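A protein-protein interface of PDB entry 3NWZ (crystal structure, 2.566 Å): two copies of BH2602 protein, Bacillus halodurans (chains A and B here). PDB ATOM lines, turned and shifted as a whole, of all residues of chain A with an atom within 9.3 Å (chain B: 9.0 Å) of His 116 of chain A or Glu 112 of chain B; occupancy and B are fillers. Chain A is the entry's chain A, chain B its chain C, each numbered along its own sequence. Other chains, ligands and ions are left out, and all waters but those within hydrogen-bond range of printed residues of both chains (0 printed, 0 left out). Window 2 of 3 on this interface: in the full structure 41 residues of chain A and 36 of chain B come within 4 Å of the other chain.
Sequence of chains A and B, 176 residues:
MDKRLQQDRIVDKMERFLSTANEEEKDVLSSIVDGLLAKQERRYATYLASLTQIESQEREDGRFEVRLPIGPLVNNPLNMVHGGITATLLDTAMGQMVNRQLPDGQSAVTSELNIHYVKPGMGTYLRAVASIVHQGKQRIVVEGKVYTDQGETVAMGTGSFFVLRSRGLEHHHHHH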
ATOM      1  N   GLY A  83     -19.732 -14.884  -5.843  1.00  0.00           N
ATOM      2  CA  GLY A  83     -20.834 -13.990  -5.515  1.00  0.00           C
ATOM      3  C   GLY A  83     -20.352 -12.586  -5.228  1.00  0.00           C
ATOM      4  O   GLY A  83     -21.082 -11.607  -5.402  1.00  0.00           O
ATOM      5  N   THR A  86     -19.664 -10.722  -8.432  1.00  0.00           N
ATOM      6  CA  THR A  86     -20.954 -10.364  -8.987  1.00  0.00           C
ATOM      7  C   THR A  86     -21.421  -9.052  -8.361  1.00  0.00           C
ATOM      8  O   THR A  86     -21.800  -8.101  -9.076  1.00  0.00           O
ATOM      9  CB  THR A  86     -22.020 -11.431  -8.714  1.00  0.00           C
ATOM     10  OG1 THR A  86     -21.574 -12.703  -9.196  1.00  0.00           O
ATOM     11  CG2 THR A  86     -23.314 -11.046  -9.434  1.00  0.00           C
ATOM     12  N   ALA A  87     -21.394  -9.009  -7.027  1.00  0.00           N
ATOM     13  CA  ALA A  87     -21.799  -7.817  -6.277  1.00  0.00           C
ATOM     14  C   ALA A  87     -20.962  -6.635  -6.682  1.00  0.00           C
ATOM     15  O   ALA A  87     -21.473  -5.582  -7.053  1.00  0.00           O
ATOM     16  CB  ALA A  87     -21.643  -8.068  -4.811  1.00  0.00           C
ATOM     17  N   LEU A  90     -22.043  -5.246 -10.116  1.00  0.00           N
ATOM     18  CA  LEU A  90     -23.283  -4.478 -10.080  1.00  0.00           C
ATOM     19  C   LEU A  90     -22.964  -3.110  -9.504  1.00  0.00           C
ATOM     20  O   LEU A  90     -23.334  -2.086 -10.066  1.00  0.00           O
ATOM     21  CB  LEU A  90     -24.326  -5.184  -9.200  1.00  0.00           C
ATOM     22  CG  LEU A  90     -25.649  -5.576  -9.864  1.00  0.00           C
ATOM     23  CD1 LEU A  90     -26.571  -6.156  -8.826  1.00  0.00           C
ATOM     24  CD2 LEU A  90     -26.295  -4.353 -10.518  1.00  0.00           C
ATOM     25  N   LEU A 113     -26.584  -1.217  -0.615  1.00  0.00           N
ATOM     26  CA  LEU A 113     -26.427  -2.164  -1.709  1.00  0.00           C
ATOM     27  C   LEU A 113     -27.301  -3.346  -1.348  1.00  0.00           C
ATOM     28  O   LEU A 113     -27.289  -3.794  -0.205  1.00  0.00           O
ATOM     29  CB  LEU A 113     -24.964  -2.598  -1.836  1.00  0.00           C
ATOM     30  CG  LEU A 113     -24.626  -3.488  -3.042  1.00  0.00           C
ATOM     31  CD1 LEU A 113     -25.043  -2.803  -4.360  1.00  0.00           C
ATOM     32  CD2 LEU A 113     -23.135  -3.765  -3.042  1.00  0.00           C
ATOM     33  N   ASN A 114     -28.079  -3.831  -2.306  1.00  0.00           N
ATOM     34  CA  ASN A 114     -28.979  -4.964  -2.082  1.00  0.00           C
ATOM     35  C   ASN A 114     -28.899  -5.819  -3.316  1.00  0.00           C
ATOM     36  O   ASN A 114     -28.908  -5.320  -4.435  1.00  0.00           O
ATOM     37  CB  ASN A 114     -30.412  -4.498  -1.893  1.00  0.00           C
ATOM     38  CG  ASN A 114     -31.268  -5.523  -1.153  1.00  0.00           C
ATOM     39  OD1 ASN A 114     -31.327  -6.711  -1.513  1.00  0.00           O
ATOM     40  ND2 ASN A 114     -31.944  -5.061  -0.110  1.00  0.00           N
ATOM     41  N   ILE A 115     -28.814  -7.125  -3.114  1.00  0.00           N
ATOM     42  CA  ILE A 115     -28.665  -8.047  -4.220  1.00  0.00           C
ATOM     43  C   ILE A 115     -29.412  -9.359  -3.953  1.00  0.00           C
ATOM     44  O   ILE A 115     -29.476  -9.841  -2.825  1.00  0.00           O
ATOM     45  CB  ILE A 115     -27.171  -8.331  -4.458  1.00  0.00           C
ATOM     46  CG1 ILE A 115     -26.358  -7.058  -4.216  1.00  0.00           C
ATOM     47  CG2 ILE A 115     -26.944  -8.774  -5.898  1.00  0.00           C
ATOM     48  CD1 ILE A 115     -24.853  -7.276  -4.142  1.00  0.00           C
ATOM     49  N   HIS A 116     -29.997  -9.907  -5.010  1.00  0.00           N
ATOM     50  CA  HIS A 116     -30.738 -11.156  -4.946  1.00  0.00           C
ATOM     51  C   HIS A 116     -30.066 -12.052  -5.958  1.00  0.00           C
ATOM     52  O   HIS A 116     -29.998 -11.716  -7.137  1.00  0.00           O
ATOM     53  CB  HIS A 116     -32.215 -10.922  -5.312  1.00  0.00           C
ATOM     54  CG  HIS A 116     -32.949 -10.096  -4.306  1.00  0.00           C
ATOM     55  ND1 HIS A 116     -33.889 -10.628  -3.454  1.00  0.00           N
ATOM     56  CD2 HIS A 116     -32.806  -8.800  -3.942  1.00  0.00           C
ATOM     57  CE1 HIS A 116     -34.289  -9.699  -2.603  1.00  0.00           C
ATOM     58  NE2 HIS A 116     -33.646  -8.580  -2.878  1.00  0.00           N
ATOM     59  N   TYR A 117     -29.526 -13.166  -5.494  1.00  0.00           N
ATOM     60  CA  TYR A 117     -28.845 -14.088  -6.381  1.00  0.00           C
ATOM     61  C   TYR A 117     -29.880 -14.992  -6.999  1.00  0.00           C
ATOM     62  O   TYR A 117     -30.743 -15.517  -6.311  1.00  0.00           O
ATOM     63  CB  TYR A 117     -27.811 -14.884  -5.601  1.00  0.00           C
ATOM     64  CG  TYR A 117     -26.642 -14.028  -5.205  1.00  0.00           C
ATOM     65  CD1 TYR A 117     -25.586 -13.803  -6.091  1.00  0.00           C
ATOM     66  CD2 TYR A 117     -26.622 -13.385  -3.968  1.00  0.00           C
ATOM     67  CE1 TYR A 117     -24.529 -12.944  -5.756  1.00  0.00           C
ATOM     68  CE2 TYR A 117     -25.579 -12.532  -3.627  1.00  0.00           C
ATOM     69  CZ  TYR A 117     -24.539 -12.316  -4.525  1.00  0.00           C
ATOM     70  OH  TYR A 117     -23.531 -11.453  -4.183  1.00  0.00           O
ATOM     71  N   VAL A 118     -29.772 -15.182  -8.307  1.00  0.00           N
ATOM     72  CA  VAL A 118     -30.749 -15.963  -9.038  1.00  0.00           C
ATOM     73  C   VAL A 118     -30.169 -17.214  -9.669  1.00  0.00           C
ATOM     74  O   VAL A 118     -30.574 -18.325  -9.336  1.00  0.00           O
ATOM     75  CB  VAL A 118     -31.392 -15.068 -10.119  1.00  0.00           C
ATOM     76  CG1 VAL A 118     -32.243 -15.896 -11.056  1.00  0.00           C
ATOM     77  CG2 VAL A 118     -32.200 -13.963  -9.447  1.00  0.00           C
ATOM     78  N   LYS A 119     -29.232 -17.024 -10.590  1.00  0.00           N
ATOM     79  CA  LYS A 119     -28.594 -18.132 -11.281  1.00  0.00           C
ATOM     80  C   LYS A 119     -27.079 -18.017 -11.175  1.00  0.00           C
ATOM     81  O   LYS A 119     -26.530 -16.913 -11.094  1.00  0.00           O
ATOM     82  CB  LYS A 119     -29.002 -18.156 -12.761  1.00  0.00           C
ATOM     83  CG  LYS A 119     -30.400 -18.701 -13.023  1.00  0.00           C
ATOM     84  CD  LYS A 119     -30.726 -18.765 -14.515  1.00  0.00           C
ATOM     85  CE  LYS A 119     -30.852 -17.374 -15.116  1.00  0.00           C
ATOM     86  NZ  LYS A 119     -31.984 -16.614 -14.519  1.00  0.00           N
ATOM     87  N   PRO A 120     -26.383 -19.162 -11.172  1.00  0.00           N
ATOM     88  CA  PRO A 120     -24.924 -19.209 -11.079  1.00  0.00           C
ATOM     89  C   PRO A 120     -24.300 -18.414 -12.208  1.00  0.00           C
ATOM     90  O   PRO A 120     -24.642 -18.632 -13.374  1.00  0.00           O
ATOM     91  CB  PRO A 120     -24.616 -20.694 -11.230  1.00  0.00           C
ATOM     92  CG  PRO A 120     -25.845 -21.350 -10.664  1.00  0.00           C
ATOM     93  CD  PRO A 120     -26.942 -20.522 -11.266  1.00  0.00           C
ATOM     94  N   GLY A 144     -30.093  -2.387 -10.871  1.00  0.00           N
ATOM     95  CA  GLY A 144     -29.359  -3.097 -11.908  1.00  0.00           C
ATOM     96  C   GLY A 144     -29.539  -4.609 -11.968  1.00  0.00           C
ATOM     97  O   GLY A 144     -30.117  -5.217 -11.082  1.00  0.00           O
ATOM     98  N   LYS A 145     -29.033  -5.213 -13.034  1.00  0.00           N
ATOM     99  CA  LYS A 145     -29.112  -6.648 -13.235  1.00  0.00           C
ATOM    100  C   LYS A 145     -27.814  -7.153 -13.833  1.00  0.00           C
ATOM    101  O   LYS A 145     -27.097  -6.420 -14.530  1.00  0.00           O
ATOM    102  CB  LYS A 145     -30.263  -7.007 -14.175  1.00  0.00           C
ATOM    103  CG  LYS A 145     -31.608  -7.066 -13.489  1.00  0.00           C
ATOM    104  CD  LYS A 145     -32.708  -7.467 -14.464  1.00  0.00           C
ATOM    105  CE  LYS A 145     -34.049  -7.574 -13.757  1.00  0.00           C
ATOM    106  NZ  LYS A 145     -34.435  -6.270 -13.141  1.00  0.00           N
ATOM    107  N   VAL A 146     -27.507  -8.409 -13.534  1.00  0.00           N
ATOM    108  CA  VAL A 146     -26.313  -9.048 -14.047  1.00  0.00           C
ATOM    109  C   VAL A 146     -26.789 -10.209 -14.931  1.00  0.00           C
ATOM    110  O   VAL A 146     -27.644 -10.990 -14.527  1.00  0.00           O
ATOM    111  CB  VAL A 146     -25.418  -9.581 -12.886  1.00  0.00           C
ATOM    112  CG1 VAL A 146     -24.177 -10.224 -13.445  1.00  0.00           C
ATOM    113  CG2 VAL A 146     -25.037  -8.448 -11.955  1.00  0.00           C
ATOM    114  N   THR A 153     -30.431 -14.214 -16.220  1.00  0.00           N
ATOM    115  CA  THR A 153     -30.185 -13.283 -15.119  1.00  0.00           C
ATOM    116  C   THR A 153     -29.450 -13.936 -13.942  1.00  0.00           C
ATOM    117  O   THR A 153     -30.028 -14.727 -13.194  1.00  0.00           O
ATOM    118  CB  THR A 153     -31.513 -12.654 -14.589  1.00  0.00           C
ATOM    119  OG1 THR A 153     -32.119 -11.839 -15.610  1.00  0.00           O
ATOM    120  CG2 THR A 153     -31.237 -11.789 -13.355  1.00  0.00           C
ATOM    121  N   VAL A 154     -28.171 -13.597 -13.790  1.00  0.00           N
ATOM    122  CA  VAL A 154     -27.346 -14.114 -12.710  1.00  0.00           C
ATOM    123  C   VAL A 154     -27.792 -13.499 -11.393  1.00  0.00           C
ATOM    124  O   VAL A 154     -27.893 -14.187 -10.374  1.00  0.00           O
ATOM    125  CB  VAL A 154     -25.857 -13.769 -12.937  1.00  0.00           C
ATOM    126  CG1 VAL A 154     -25.011 -14.200 -11.728  1.00  0.00           C
ATOM    127  CG2 VAL A 154     -25.372 -14.430 -14.208  1.00  0.00           C
ATOM    128  N   ALA A 155     -28.064 -12.201 -11.409  1.00  0.00           N
ATOM    129  CA  ALA A 155     -28.506 -11.539 -10.195  1.00  0.00           C
ATOM    130  C   ALA A 155     -29.202 -10.225 -10.454  1.00  0.00           C
ATOM    131  O   ALA A 155     -29.039  -9.601 -11.497  1.00  0.00           O
ATOM    132  CB  ALA A 155     -27.334 -11.314  -9.268  1.00  0.00           C
ATOM    133  N   MET A 156     -29.976  -9.800  -9.466  1.00  0.00           N
ATOM    134  CA  MET A 156     -30.721  -8.549  -9.540  1.00  0.00           C
ATOM    135  C   MET A 156     -30.498  -7.840  -8.191  1.00  0.00           C
ATOM    136  O   MET A 156     -30.330  -8.514  -7.169  1.00  0.00           O
ATOM    137  CB  MET A 156     -32.189  -8.902  -9.769  1.00  0.00           C
ATOM    138  CG  MET A 156     -33.060  -7.796 -10.275  1.00  0.00           C
ATOM    139  SD  MET A 156     -33.991  -6.918  -8.857  1.00  0.00           S
ATOM    140  CE  MET A 156     -33.517  -5.094  -9.361  1.00  0.00           C
ATOM    141  N   GLY A 157     -30.452  -6.504  -8.197  1.00  0.00           N
ATOM    142  CA  GLY A 157     -30.264  -5.747  -6.970  1.00  0.00           C
ATOM    143  C   GLY A 157     -30.453  -4.230  -7.080  1.00  0.00           C
ATOM    144  O   GLY A 157     -30.557  -3.684  -8.172  1.00  0.00           O
ATOM    145  N   THR A 158     -30.507  -3.544  -5.940  1.00  0.00           N
ATOM    146  CA  THR A 158     -30.653  -2.092  -5.926  1.00  0.00           C
ATOM    147  C   THR A 158     -29.517  -1.481  -5.098  1.00  0.00           C
ATOM    148  O   THR A 158     -28.864  -2.162  -4.306  1.00  0.00           O
ATOM    149  CB  THR A 158     -32.036  -1.644  -5.321  1.00  0.00           C
ATOM    150  OG1 THR A 158     -32.141  -2.099  -3.964  1.00  0.00           O
ATOM    151  CG2 THR A 158     -33.226  -2.266  -6.132  1.00  0.00           C
ATOM    152  N   ASP B  91     -19.655 -11.205   3.074  1.00  0.00           N
ATOM    153  CA  ASP B  91     -20.275 -12.420   2.552  1.00  0.00           C
ATOM    154  C   ASP B  91     -19.473 -13.674   2.905  1.00  0.00           C
ATOM    155  O   ASP B  91     -20.022 -14.774   3.009  1.00  0.00           O
ATOM    156  CB  ASP B  91     -20.433 -12.323   1.031  1.00  0.00           C
ATOM    157  CG  ASP B  91     -20.878 -13.624   0.413  1.00  0.00           C
ATOM    158  OD1 ASP B  91     -21.904 -14.174   0.860  1.00  0.00           O
ATOM    159  OD2 ASP B  91     -20.200 -14.102  -0.519  1.00  0.00           O
ATOM    160  N   MET B  94     -20.100 -14.438   6.922  1.00  0.00           N
ATOM    161  CA  MET B  94     -21.420 -15.044   7.090  1.00  0.00           C
ATOM    162  C   MET B  94     -21.560 -16.307   6.262  1.00  0.00           C
ATOM    163  O   MET B  94     -22.337 -17.197   6.588  1.00  0.00           O
ATOM    164  CB  MET B  94     -22.511 -14.082   6.644  1.00  0.00           C
ATOM    165  CG  MET B  94     -22.424 -12.684   7.188  1.00  0.00           C
ATOM    166  SD  MET B  94     -23.863 -11.655   6.406  1.00  0.00           S
ATOM    167  CE  MET B  94     -23.260 -11.738   4.571  1.00  0.00           C
ATOM    168  N   VAL B 109     -25.666 -21.602  -0.431  1.00  0.00           N
ATOM    169  CA  VAL B 109     -25.216 -20.553  -1.326  1.00  0.00           C
ATOM    170  C   VAL B 109     -25.885 -19.246  -0.914  1.00  0.00           C
ATOM    171  O   VAL B 109     -26.988 -19.255  -0.369  1.00  0.00           O
ATOM    172  CB  VAL B 109     -25.586 -20.879  -2.774  1.00  0.00           C
ATOM    173  CG1 VAL B 109     -24.724 -22.026  -3.267  1.00  0.00           C
ATOM    174  CG2 VAL B 109     -27.068 -21.249  -2.863  1.00  0.00           C
ATOM    175  N   THR B 110     -25.211 -18.126  -1.160  1.00  0.00           N
ATOM    176  CA  THR B 110     -25.761 -16.824  -0.803  1.00  0.00           C
ATOM    177  C   THR B 110     -26.966 -16.524  -1.695  1.00  0.00           C
ATOM    178  O   THR B 110     -26.888 -16.592  -2.928  1.00  0.00           O
ATOM    179  CB  THR B 110     -24.732 -15.696  -0.965  1.00  0.00           C
ATOM    180  OG1 THR B 110     -23.538 -16.028  -0.250  1.00  0.00           O
ATOM    181  CG2 THR B 110     -25.296 -14.412  -0.403  1.00  0.00           C
ATOM    182  N   SER B 111     -28.066 -16.181  -1.039  1.00  0.00           N
ATOM    183  CA  SER B 111     -29.341 -15.906  -1.677  1.00  0.00           C
ATOM    184  C   SER B 111     -29.623 -14.393  -1.703  1.00  0.00           C
ATOM    185  O   SER B 111     -29.878 -13.820  -2.779  1.00  0.00           O
ATOM    186  CB  SER B 111     -30.428 -16.665  -0.900  1.00  0.00           C
ATOM    187  OG  SER B 111     -31.727 -16.409  -1.377  1.00  0.00           O
ATOM    188  N   GLU B 112     -29.582 -13.762  -0.527  1.00  0.00           N
ATOM    189  CA  GLU B 112     -29.806 -12.319  -0.383  1.00  0.00           C
ATOM    190  C   GLU B 112     -28.657 -11.662   0.361  1.00  0.00           C
ATOM    191  O   GLU B 112     -28.176 -12.196   1.347  1.00  0.00           O
ATOM    192  CB  GLU B 112     -31.080 -12.009   0.425  1.00  0.00           C
ATOM    193  CG  GLU B 112     -32.375 -11.927  -0.344  1.00  0.00           C
ATOM    194  CD  GLU B 112     -32.834 -13.280  -0.812  1.00  0.00           C
ATOM    195  OE1 GLU B 112     -32.840 -14.220   0.017  1.00  0.00           O
ATOM    196  OE2 GLU B 112     -33.194 -13.403  -2.005  1.00  0.00           O
ATOM    197  N   LEU B 113     -28.231 -10.492  -0.100  1.00  0.00           N
ATOM    198  CA  LEU B 113     -27.180  -9.783   0.581  1.00  0.00           C
ATOM    199  C   LEU B 113     -27.531  -8.313   0.697  1.00  0.00           C
ATOM    200  O   LEU B 113     -27.676  -7.620  -0.305  1.00  0.00           O
ATOM    201  CB  LEU B 113     -25.844  -9.952  -0.139  1.00  0.00           C
ATOM    202  CG  LEU B 113     -24.664  -9.296   0.589  1.00  0.00           C
ATOM    203  CD1 LEU B 113     -24.650  -9.736   2.047  1.00  0.00           C
ATOM    204  CD2 LEU B 113     -23.363  -9.673  -0.100  1.00  0.00           C
ATOM    205  N   ASN B 114     -27.679  -7.851   1.937  1.00  0.00           N
ATOM    206  CA  ASN B 114     -27.989  -6.462   2.216  1.00  0.00           C
ATOM    207  C   ASN B 114     -26.859  -5.835   3.027  1.00  0.00           C
ATOM    208  O   ASN B 114     -26.490  -6.338   4.085  1.00  0.00           O
ATOM    209  CB  ASN B 114     -29.273  -6.353   3.012  1.00  0.00           C
ATOM    210  CG  ASN B 114     -29.863  -4.958   2.951  1.00  0.00           C
ATOM    211  OD1 ASN B 114     -29.209  -3.974   3.288  1.00  0.00           O
ATOM    212  ND2 ASN B 114     -31.109  -4.867   2.510  1.00  0.00           N
ATOM    213  N   ILE B 115     -26.323  -4.721   2.543  1.00  0.00           N
ATOM    214  CA  ILE B 115     -25.233  -4.056   3.234  1.00  0.00           C
ATOM    215  C   ILE B 115     -25.391  -2.540   3.332  1.00  0.00           C
ATOM    216  O   ILE B 115     -25.823  -1.877   2.387  1.00  0.00           O
ATOM    217  CB  ILE B 115     -23.883  -4.414   2.551  1.00  0.00           C
ATOM    218  CG1 ILE B 115     -23.537  -5.864   2.864  1.00  0.00           C
ATOM    219  CG2 ILE B 115     -22.762  -3.511   3.042  1.00  0.00           C
ATOM    220  CD1 ILE B 115     -22.243  -6.318   2.251  1.00  0.00           C
ATOM    221  N   ARG B 139     -33.722 -21.865   4.605  1.00  0.00           N
ATOM    222  CA  ARG B 139     -32.645 -20.866   4.567  1.00  0.00           C
ATOM    223  C   ARG B 139     -32.153 -20.443   5.953  1.00  0.00           C
ATOM    224  O   ARG B 139     -32.853 -20.621   6.954  1.00  0.00           O
ATOM    225  CB  ARG B 139     -33.077 -19.619   3.758  1.00  0.00           C
ATOM    226  CG  ARG B 139     -34.382 -18.924   4.192  1.00  0.00           C
ATOM    227  CD  ARG B 139     -34.272 -18.220   5.545  1.00  0.00           C
ATOM    228  NE  ARG B 139     -35.425 -17.363   5.825  1.00  0.00           N
ATOM    229  CZ  ARG B 139     -35.522 -16.100   5.427  1.00  0.00           C
ATOM    230  NH1 ARG B 139     -34.534 -15.552   4.737  1.00  0.00           N
ATOM    231  NH2 ARG B 139     -36.597 -15.383   5.712  1.00  0.00           N
ATOM    232  N   ILE B 140     -30.939 -19.896   6.007  1.00  0.00           N
ATOM    233  CA  ILE B 140     -30.352 -19.422   7.269  1.00  0.00           C
ATOM    234  C   ILE B 140     -30.045 -17.926   7.163  1.00  0.00           C
ATOM    235  O   ILE B 140     -29.176 -17.522   6.394  1.00  0.00           O
ATOM    236  CB  ILE B 140     -29.009 -20.166   7.615  1.00  0.00           C
ATOM    237  CG1 ILE B 140     -29.261 -21.659   7.813  1.00  0.00           C
ATOM    238  CG2 ILE B 140     -28.361 -19.559   8.867  1.00  0.00           C
ATOM    239  CD1 ILE B 140     -29.411 -22.410   6.518  1.00  0.00           C
ATOM    240  N   VAL B 141     -30.764 -17.105   7.918  1.00  0.00           N
ATOM    241  CA  VAL B 141     -30.503 -15.672   7.896  1.00  0.00           C
ATOM    242  C   VAL B 141     -29.351 -15.397   8.851  1.00  0.00           C
ATOM    243  O   VAL B 141     -29.279 -15.981   9.933  1.00  0.00           O
ATOM    244  CB  VAL B 141     -31.713 -14.852   8.358  1.00  0.00           C
ATOM    245  CG1 VAL B 141     -31.369 -13.370   8.349  1.00  0.00           C
ATOM    246  CG2 VAL B 141     -32.900 -15.139   7.459  1.00  0.00           C
ATOM    247  N   VAL B 142     -28.451 -14.509   8.442  1.00  0.00           N
ATOM    248  CA  VAL B 142     -27.304 -14.153   9.245  1.00  0.00           C
ATOM    249  C   VAL B 142     -26.993 -12.646   9.158  1.00  0.00           C
ATOM    250  O   VAL B 142     -27.044 -12.058   8.089  1.00  0.00           O
ATOM    251  CB  VAL B 142     -26.092 -14.969   8.776  1.00  0.00           C
ATOM    252  CG1 VAL B 142     -25.887 -14.752   7.304  1.00  0.00           C
ATOM    253  CG2 VAL B 142     -24.846 -14.577   9.563  1.00  0.00           C
ATOM    254  N   GLY B 157     -24.453  -5.280   7.788  1.00  0.00           N
ATOM    255  CA  GLY B 157     -25.379  -5.900   6.856  1.00  0.00           C
ATOM    256  C   GLY B 157     -25.910  -7.281   7.202  1.00  0.00           C
ATOM    257  O   GLY B 157     -25.283  -8.049   7.935  1.00  0.00           O
ATOM    258  N   THR B 158     -27.083  -7.597   6.662  1.00  0.00           N
ATOM    259  CA  THR B 158     -27.697  -8.903   6.874  1.00  0.00           C
ATOM    260  C   THR B 158     -27.551  -9.708   5.576  1.00  0.00           C
ATOM    261  O   THR B 158     -27.236  -9.159   4.528  1.00  0.00           O
ATOM    262  CB  THR B 158     -29.182  -8.768   7.268  1.00  0.00           C
ATOM    263  OG1 THR B 158     -29.977  -8.545   6.100  1.00  0.00           O
ATOM    264  CG2 THR B 158     -29.368  -7.577   8.224  1.00  0.00           C
ATOM    265  N   GLY B 159     -27.758 -11.013   5.662  1.00  0.00           N
ATOM    266  CA  GLY B 159     -27.622 -11.877   4.512  1.00  0.00           C
ATOM    267  C   GLY B 159     -28.478 -13.137   4.658  1.00  0.00           C
ATOM    268  O   GLY B 159     -28.715 -13.616   5.774  1.00  0.00           O
ATOM    269  N   SER B 160     -28.967 -13.668   3.534  1.00  0.00           N
ATOM    270  CA  SER B 160     -29.772 -14.877   3.575  1.00  0.00           C
ATOM    271  C   SER B 160     -29.071 -15.958   2.776  1.00  0.00           C
ATOM    272  O   SER B 160     -28.565 -15.719   1.678  1.00  0.00           O
ATOM    273  CB  SER B 160     -31.169 -14.638   3.024  1.00  0.00           C
ATOM    274  OG  SER B 160     -32.019 -15.716   3.392  1.00  0.00           O
ATOM    275  N   PHE B 161     -29.028 -17.151   3.354  1.00  0.00           N
ATOM    276  CA  PHE B 161     -28.360 -18.265   2.725  1.00  0.00           C
ATOM    277  C   PHE B 161     -29.321 -19.410   2.468  1.00  0.00           C
ATOM    278  O   PHE B 161     -30.133 -19.766   3.328  1.00  0.00           O
ATOM    279  CB  PHE B 161     -27.178 -18.691   3.598  1.00  0.00           C
ATOM    280  CG  PHE B 161     -26.065 -17.680   3.624  1.00  0.00           C
ATOM    281  CD1 PHE B 161     -24.913 -17.878   2.883  1.00  0.00           C
ATOM    282  CD2 PHE B 161     -26.193 -16.505   4.340  1.00  0.00           C
ATOM    283  CE1 PHE B 161     -23.908 -16.921   2.853  1.00  0.00           C
ATOM    284  CE2 PHE B 161     -25.188 -15.541   4.312  1.00  0.00           C
ATOM    285  CZ  PHE B 161     -24.049 -15.751   3.568  1.00  0.00           C
ATOM    286  N   PHE B 162     -29.228 -19.964   1.264  1.00  0.00           N
ATOM    287  CA  PHE B 162     -30.094 -21.049   0.825  1.00  0.00           C
ATOM    288  C   PHE B 162     -29.388 -22.374   1.043  1.00  0.00           C
ATOM    289  O   PHE B 162     -28.199 -22.491   0.769  1.00  0.00           O
ATOM    290  CB  PHE B 162     -30.404 -20.866  -0.667  1.00  0.00           C
ATOM    291  CG  PHE B 162     -31.644 -21.576  -1.135  1.00  0.00           C
ATOM    292  CD1 PHE B 162     -32.905 -21.122  -0.761  1.00  0.00           C
ATOM    293  CD2 PHE B 162     -31.553 -22.674  -1.987  1.00  0.00           C
ATOM    294  CE1 PHE B 162     -34.059 -21.749  -1.236  1.00  0.00           C
ATOM    295  CE2 PHE B 162     -32.697 -23.308  -2.468  1.00  0.00           C
ATOM    296  CZ  PHE B 162     -33.951 -22.848  -2.096  1.00  0.00           C
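The backbone NH (N) of Tyr 117 of chain A sits at hydrogen-bond distance from the backbone carbonyl oxygen (O) of Ser 111 of chain B (2.8 Å). The backbone NH of Ile 115 of chain B lies within hydrogen-bond range of the backbone carbonyl oxygen of Leu 113 of chain A, at 3.1 Å. N of Leu 113 of chain B sits at hydrogen-bond distance from O of Ile 115 of chain A (3.1 Å). ND2 of Asn 114 of chain A sits close to ND2 of Asn 114 of chain B (2.8 Å). A ring nitrogen (ND1) of His 116 of chain A lies within hydrogen-bond range of the side-chain carboxylate (OE2) of Glu 112 of chain B (3.2 Å).
O of Asn 114 of chain B lies within hydrogen-bond range of N of Thr 158 of chain B. OE1 of Glu 112 of chain B lies within hydrogen-bond range of OG of Ser 111 of chain B. OD1 of Asp 91 of chain B lies within hydrogen-bond range of OG1 of Thr 110 of chain B, 2.7 Å away. The backbone NH of His 116 of chain A is in hydrogen-bond range of the backbone carbonyl oxygen of Met 156 of chain A (2.6 Å). The side-chain amide oxygen of Asn 114 of chain A is in hydrogen-bond range of a ring nitrogen (NE2) of His 116 of chain A.
Among the printed residues, merely in contact across the chains: Tyr 117 of chain A with Thr 110 of chain B (3.3 Å), Asn 114 of chain A with Leu 113 of chain B (3.5 Å), Ile 115 of chain A with Glu 112 of chain B (3.5 Å), His 116 of chain A with Ser 111 of chain B (3.5 Å), Leu 113 of chain A with Asn 114 of chain B (3.7 Å), Leu 113 of chain A with Leu 113 of chain B (3.8 Å) and Ile 115 of chain A with Ser 111 of chain B (3.9995 Å).
Printed residues of chain B within 4 Å of His 116 of chain A: Ser 111 and Glu 112. Of chain A, only Ile 115 and His 116 come within 4 Å of Glu 112 of chain B. No residue of chain B comes within 4 Å of Ala 155 of chain A. No residue of chain A comes within 4 Å of Gly 159 of chain B. No residue of chain A comes within 4 Å of Ser 160 of chain B. Printed residues of chain B within 4 Å of Ile 115 of chain A: Ser 111 (3.9995 Å), Glu 112 (3.5 Å) and Leu 113 (3.1 Å). Of the printed residues of chain B, Leu 113 of chain A touches Leu 113 (3.8 Å), Asn 114 (3.7 Å) and Ile 115 (3.1 Å). Gly 144 of chain A touches none of the printed residues of chain B. Val 142 of chain B touches none of the printed residues of chain A. The nearest residue of chain A that does not touch Glu 112 of chain B is Tyr 117 of chain A (4.6 Å). The nearest printed residue of chain A that does not touch Ser 111 of chain B is Val 118 of chain A (5.7 Å).
Of the 21 printed residues of chain A, 5 touch a printed residue of chain B. Hydrophobic or aromatic side chains of chain A that line the printed part of chain B: His 116 and Tyr 117. Along chain B the printed residues that touch a printed residue of chain A span positions 110 to 115. Among the printed residues, 12 pairs touch across the chains. Among the printed residues, no Asp or Glu carboxylate lies within 4 Å of a Lys or Arg side-chain nitrogen of the other chain.
Leu 113 of chain A touches its own counterpart, Leu 113 of chain B. Leu 113 of chain A touches Asn 114 of chain B, and with the chains exchanged Asn 114 of chain A touches Leu 113 of chain B. Leu 113 of chain A touches Ile 115 of chain B, and with the chains exchanged Ile 115 of chain A touches Leu 113 of chain B. Asn 114 of chain A touches its own counterpart, Asn 114 of chain B. Positions printed for both chains: 113, 114, 115, 157 and 158. Of the 12 pairs that touch across the chains among the printed residues, 6 have their exchanged pair printed and touching as well.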
